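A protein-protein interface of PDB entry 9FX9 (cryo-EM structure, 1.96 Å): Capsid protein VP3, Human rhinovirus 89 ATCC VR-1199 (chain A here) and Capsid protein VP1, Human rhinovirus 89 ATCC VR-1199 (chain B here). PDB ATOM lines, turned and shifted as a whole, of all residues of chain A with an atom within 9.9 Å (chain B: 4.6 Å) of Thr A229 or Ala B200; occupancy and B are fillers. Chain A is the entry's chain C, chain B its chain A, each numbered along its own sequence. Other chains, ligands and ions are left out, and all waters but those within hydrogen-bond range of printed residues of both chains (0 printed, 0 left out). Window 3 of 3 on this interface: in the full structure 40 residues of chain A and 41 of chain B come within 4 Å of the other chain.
O of Val B199 lies within hydrogen-bond range of NE2 of His A228.
The backbone carbonyl oxygen of Val B199 sits at hydrogen-bond distance from the guanidinium group of Arg B197 (2.9 Å).
The guanidinium group of Arg B197 lies within hydrogen-bond range of the backbone carbonyl oxygen of Ala B200, at 2.8 Å.
NH1 of Arg B197 sits at hydrogen-bond distance from O of Asn B208, 2.8 Å away.
His A228 touches Arg B197.
His A228 touches Ala B200 (NE2 to CA, 3.96 Å).
Tyr B201 touches His A228 (CD2 to CE1, 3.8 Å).
Thr A229 touches Ala B200.
Printed residues of chain B within 4 Å of Thr A229: Ala B200.
Of the printed residues of chain A, Ala B200 touches His A228 (3.96 Å) and Thr A229 (3.99 Å).
Of chain A, only His A228 (2.9 Å) comes within 4 Å of Val B199.
Printed residues of chain A within 4 Å of Tyr B201: His A228 (3.8 Å).
Of the printed residues of chain A, Arg B197 touches His A228 (3.5 Å).
Printed residues of chain B within 4 Å of His A228: Arg B197, Val B199, Ala B200 and Tyr B201.
Tyr A103 touches none of the printed residues of chain B.
Arg A61 touches none of the printed residues of chain B.
The nearest printed residue of chain A that does not touch Ala B200 is Leu A227 (8.7 Å).
The nearest printed residue of chain A that does not touch Tyr B201 is Thr A229 (5.9 Å).
Printed residues of chain B that touch a printed residue of chain A: Arg B197, Val B199, Ala B200 and Tyr B201.
Hydrophobic or aromatic side chains of chain B within 4 Å of the printed part of chain A: Ala B200 and Tyr B201.
Along chain B the printed residues that touch a printed residue of chain A span positions 197 to 201.
Hydrophobic or aromatic side chains of chain A that line the printed part of chain B: His A228.
Among the printed residues, no Asp or Glu carboxylate lies within 4 Å of a Lys or Arg side-chain nitrogen of the other chain.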
ATOM      1  N   ARG A  61      -6.762   5.672  39.326  1.00  0.00           N
ATOM      2  CA  ARG A  61      -7.609   5.460  38.133  1.00  0.00           C
ATOM      3  C   ARG A  61      -8.533   6.652  37.827  1.00  0.00           C
ATOM      4  O   ARG A  61      -9.586   6.476  37.219  1.00  0.00           O
ATOM      5  CB  ARG A  61      -8.396   4.138  38.284  1.00  0.00           C
ATOM      6  CG  ARG A  61      -7.536   2.885  38.541  1.00  0.00           C
ATOM      7  CD  ARG A  61      -6.497   2.598  37.451  1.00  0.00           C
ATOM      8  NE  ARG A  61      -7.121   2.281  36.153  1.00  0.00           N
ATOM      9  CZ  ARG A  61      -6.489   2.011  35.027  1.00  0.00           C
ATOM     10  NH1 ARG A  61      -7.150   1.706  33.951  1.00  0.00           N
ATOM     11  NH2 ARG A  61      -5.190   2.032  34.942  1.00  0.00           N
ATOM     12  N   GLU A  99       8.089  13.092  31.862  1.00  0.00           N
ATOM     13  CA  GLU A  99       7.957  12.351  30.613  1.00  0.00           C
ATOM     14  C   GLU A  99       8.997  12.784  29.579  1.00  0.00           C
ATOM     15  O   GLU A  99       9.704  11.934  29.049  1.00  0.00           O
ATOM     16  CB  GLU A  99       6.545  12.548  30.057  1.00  0.00           C
ATOM     17  CG  GLU A  99       5.495  11.741  30.831  1.00  0.00           C
ATOM     18  CD  GLU A  99       5.534  10.238  30.527  1.00  0.00           C
ATOM     19  OE1 GLU A  99       6.183   9.813  29.547  1.00  0.00           O
ATOM     20  OE2 GLU A  99       4.841   9.472  31.226  1.00  0.00           O
ATOM     21  N   TYR A 103      13.045  10.650  28.024  1.00  0.00           N
ATOM     22  CA  TYR A 103      13.699  10.463  26.719  1.00  0.00           C
ATOM     23  C   TYR A 103      15.186  10.828  26.709  1.00  0.00           C
ATOM     24  O   TYR A 103      15.845  10.725  25.677  1.00  0.00           O
ATOM     25  CB  TYR A 103      12.971  11.272  25.643  1.00  0.00           C
ATOM     26  CG  TYR A 103      11.640  10.690  25.254  1.00  0.00           C
ATOM     27  CD1 TYR A 103      11.592   9.503  24.503  1.00  0.00           C
ATOM     28  CD2 TYR A 103      10.456  11.351  25.611  1.00  0.00           C
ATOM     29  CE1 TYR A 103      10.353   8.973  24.108  1.00  0.00           C
ATOM     30  CE2 TYR A 103       9.216  10.831  25.209  1.00  0.00           C
ATOM     31  CZ  TYR A 103       9.169   9.643  24.455  1.00  0.00           C
ATOM     32  OH  TYR A 103       7.972   9.170  24.036  1.00  0.00           O
ATOM     33  N   THR A 225      13.620   3.606  25.833  1.00  0.00           N
ATOM     34  CA  THR A 225      13.497   2.491  26.796  1.00  0.00           C
ATOM     35  C   THR A 225      12.028   2.164  27.095  1.00  0.00           C
ATOM     36  O   THR A 225      11.138   2.967  26.809  1.00  0.00           O
ATOM     37  CB  THR A 225      14.292   2.812  28.077  1.00  0.00           C
ATOM     38  OG1 THR A 225      14.314   1.710  28.957  1.00  0.00           O
ATOM     39  CG2 THR A 225      13.738   3.994  28.862  1.00  0.00           C
ATOM     40  N   ASN A 226      11.750   0.993  27.673  1.00  0.00           N
ATOM     41  CA  ASN A 226      10.409   0.426  27.901  1.00  0.00           C
ATOM     42  C   ASN A 226       9.584   1.103  29.027  1.00  0.00           C
ATOM     43  O   ASN A 226       8.664   0.491  29.567  1.00  0.00           O
ATOM     44  CB  ASN A 226      10.536  -1.095  28.139  1.00  0.00           C
ATOM     45  CG  ASN A 226      11.297  -1.830  27.053  1.00  0.00           C
ATOM     46  OD1 ASN A 226      12.518  -1.874  27.048  1.00  0.00           O
ATOM     47  ND2 ASN A 226      10.620  -2.431  26.104  1.00  0.00           N
ATOM     48  N   LEU A 227       9.880   2.354  29.407  1.00  0.00           N
ATOM     49  CA  LEU A 227       9.071   3.121  30.377  1.00  0.00           C
ATOM     50  C   LEU A 227       7.658   3.436  29.837  1.00  0.00           C
ATOM     51  O   LEU A 227       6.734   3.683  30.612  1.00  0.00           O
ATOM     52  CB  LEU A 227       9.832   4.393  30.800  1.00  0.00           C
ATOM     53  CG  LEU A 227      11.085   4.113  31.657  1.00  0.00           C
ATOM     54  CD1 LEU A 227      11.903   5.394  31.812  1.00  0.00           C
ATOM     55  CD2 LEU A 227      10.733   3.608  33.055  1.00  0.00           C
ATOM     56  N   HIS A 228       7.468   3.336  28.520  1.00  0.00           N
ATOM     57  CA  HIS A 228       6.187   3.044  27.875  1.00  0.00           C
ATOM     58  C   HIS A 228       6.345   1.767  27.040  1.00  0.00           C
ATOM     59  O   HIS A 228       7.343   1.602  26.335  1.00  0.00           O
ATOM     60  CB  HIS A 228       5.733   4.249  27.040  1.00  0.00           C
ATOM     61  CG  HIS A 228       4.454   4.006  26.277  1.00  0.00           C
ATOM     62  ND1 HIS A 228       4.358   3.363  25.042  1.00  0.00           N
ATOM     63  CD2 HIS A 228       3.201   4.363  26.684  1.00  0.00           C
ATOM     64  CE1 HIS A 228       3.053   3.359  24.727  1.00  0.00           C
ATOM     65  NE2 HIS A 228       2.338   3.946  25.699  1.00  0.00           N
ATOM     66  N   THR A 229       5.393   0.841  27.133  1.00  0.00           N
ATOM     67  CA  THR A 229       5.416  -0.440  26.407  1.00  0.00           C
ATOM     68  C   THR A 229       4.937  -0.266  24.974  1.00  0.00           C
ATOM     69  O   THR A 229       5.271  -1.065  24.093  1.00  0.00           O
ATOM     70  CB  THR A 229       4.556  -1.487  27.123  1.00  0.00           C
ATOM     71  OG1 THR A 229       3.242  -1.007  27.319  1.00  0.00           O
ATOM     72  CG2 THR A 229       5.128  -1.858  28.491  1.00  0.00           C
ATOM     73  N   ALA B  49       5.771   1.260  18.441  1.00  0.00           N
ATOM     74  CA  ALA B  49       5.284   2.097  19.537  1.00  0.00           C
ATOM     75  C   ALA B  49       6.283   3.189  19.955  1.00  0.00           C
ATOM     76  O   ALA B  49       5.895   4.337  20.162  1.00  0.00           O
ATOM     77  CB  ALA B  49       4.945   1.180  20.712  1.00  0.00           C
ATOM     78  N   ARG B 197       1.456   9.930  25.323  1.00  0.00           N
ATOM     79  CA  ARG B 197       0.640   8.719  25.447  1.00  0.00           C
ATOM     80  C   ARG B 197       0.905   8.032  26.791  1.00  0.00           C
ATOM     81  O   ARG B 197       2.033   7.617  27.049  1.00  0.00           O
ATOM     82  CB  ARG B 197       0.995   7.819  24.256  1.00  0.00           C
ATOM     83  CG  ARG B 197       0.207   6.517  24.228  1.00  0.00           C
ATOM     84  CD  ARG B 197      -1.270   6.739  23.933  1.00  0.00           C
ATOM     85  NE  ARG B 197      -1.960   5.446  23.887  1.00  0.00           N
ATOM     86  CZ  ARG B 197      -3.120   5.205  23.329  1.00  0.00           C
ATOM     87  NH1 ARG B 197      -3.549   3.984  23.227  1.00  0.00           N
ATOM     88  NH2 ARG B 197      -3.879   6.162  22.891  1.00  0.00           N
ATOM     89  N   VAL B 199      -0.801   5.259  28.170  1.00  0.00           N
ATOM     90  CA  VAL B 199      -1.268   3.860  28.181  1.00  0.00           C
ATOM     91  C   VAL B 199      -0.892   3.166  26.872  1.00  0.00           C
ATOM     92  O   VAL B 199      -0.579   3.831  25.881  1.00  0.00           O
ATOM     93  CB  VAL B 199      -2.784   3.788  28.442  1.00  0.00           C
ATOM     94  CG1 VAL B 199      -3.108   4.074  29.909  1.00  0.00           C
ATOM     95  CG2 VAL B 199      -3.588   4.767  27.582  1.00  0.00           C
ATOM     96  N   ALA B 200      -0.869   1.839  26.845  1.00  0.00           N
ATOM     97  CA  ALA B 200      -0.390   1.072  25.692  1.00  0.00           C
ATOM     98  C   ALA B 200      -1.135   1.404  24.384  1.00  0.00           C
ATOM     99  O   ALA B 200      -2.335   1.684  24.375  1.00  0.00           O
ATOM    100  CB  ALA B 200      -0.491  -0.418  26.030  1.00  0.00           C
ATOM    101  N   TYR B 201      -0.426   1.380  23.257  1.00  0.00           N
ATOM    102  CA  TYR B 201      -1.049   1.373  21.933  1.00  0.00           C
ATOM    103  C   TYR B 201      -1.655  -0.001  21.636  1.00  0.00           C
ATOM    104  O   TYR B 201      -1.000  -1.023  21.832  1.00  0.00           O
ATOM    105  CB  TYR B 201      -0.030   1.749  20.856  1.00  0.00           C
ATOM    106  CG  TYR B 201       0.386   3.202  20.884  1.00  0.00           C
ATOM    107  CD1 TYR B 201      -0.572   4.201  20.635  1.00  0.00           C
ATOM    108  CD2 TYR B 201       1.723   3.556  21.126  1.00  0.00           C
ATOM    109  CE1 TYR B 201      -0.195   5.551  20.616  1.00  0.00           C
ATOM    110  CE2 TYR B 201       2.109   4.909  21.101  1.00  0.00           C
ATOM    111  CZ  TYR B 201       1.149   5.906  20.833  1.00  0.00           C
ATOM    112  OH  TYR B 201       1.510   7.208  20.803  1.00  0.00           O
ATOM    113  N   GLN B 202      -2.895  -0.020  21.150  1.00  0.00           N
ATOM    114  CA  GLN B 202      -3.578  -1.259  20.768  1.00  0.00           C
ATOM    115  C   GLN B 202      -3.499  -1.528  19.259  1.00  0.00           C
ATOM    116  O   GLN B 202      -3.192  -2.647  18.855  1.00  0.00           O
ATOM    117  CB  GLN B 202      -5.031  -1.228  21.270  1.00  0.00           C
ATOM    118  CG  GLN B 202      -5.164  -1.075  22.796  1.00  0.00           C
ATOM    119  CD  GLN B 202      -4.519  -2.195  23.616  1.00  0.00           C
ATOM    120  OE1 GLN B 202      -4.243  -3.289  23.145  1.00  0.00           O
ATOM    121  NE2 GLN B 202      -4.252  -1.971  24.882  1.00  0.00           N
ATOM    122  N   ASN B 208      -7.382   4.287  20.505  1.00  0.00           N
ATOM    123  CA  ASN B 208      -7.905   3.268  21.427  1.00  0.00           C
ATOM    124  C   ASN B 208      -6.813   2.712  22.362  1.00  0.00           C
ATOM    125  O   ASN B 208      -5.660   2.550  21.962  1.00  0.00           O
ATOM    126  CB  ASN B 208      -8.594   2.132  20.637  1.00  0.00           C
ATOM    127  CG  ASN B 208      -9.847   2.553  19.881  1.00  0.00           C
ATOM    128  OD1 ASN B 208     -10.283   3.693  19.929  1.00  0.00           O
ATOM    129  ND2 ASN B 208     -10.454   1.651  19.151  1.00  0.00           N
ATOM    130  N   TYR B 209      -7.169   2.440  23.618  1.00  0.00           N
ATOM    131  CA  TYR B 209      -6.220   2.023  24.668  1.00  0.00           C
ATOM    132  C   TYR B 209      -6.653   0.815  25.508  1.00  0.00           C
ATOM    133  O   TYR B 209      -5.803   0.192  26.140  1.00  0.00           O
ATOM    134  CB  TYR B 209      -5.914   3.214  25.584  1.00  0.00           C
ATOM    135  CG  TYR B 209      -7.109   3.857  26.250  1.00  0.00           C
ATOM    136  CD1 TYR B 209      -7.605   3.343  27.465  1.00  0.00           C
ATOM    137  CD2 TYR B 209      -7.712   4.985  25.663  1.00  0.00           C
ATOM    138  CE1 TYR B 209      -8.731   3.931  28.069  1.00  0.00           C
ATOM    139  CE2 TYR B 209      -8.833   5.574  26.264  1.00  0.00           C
ATOM    140  CZ  TYR B 209      -9.353   5.034  27.453  1.00  0.00           C
ATOM    141  OH  TYR B 209     -10.471   5.574  27.980  1.00  0.00           O
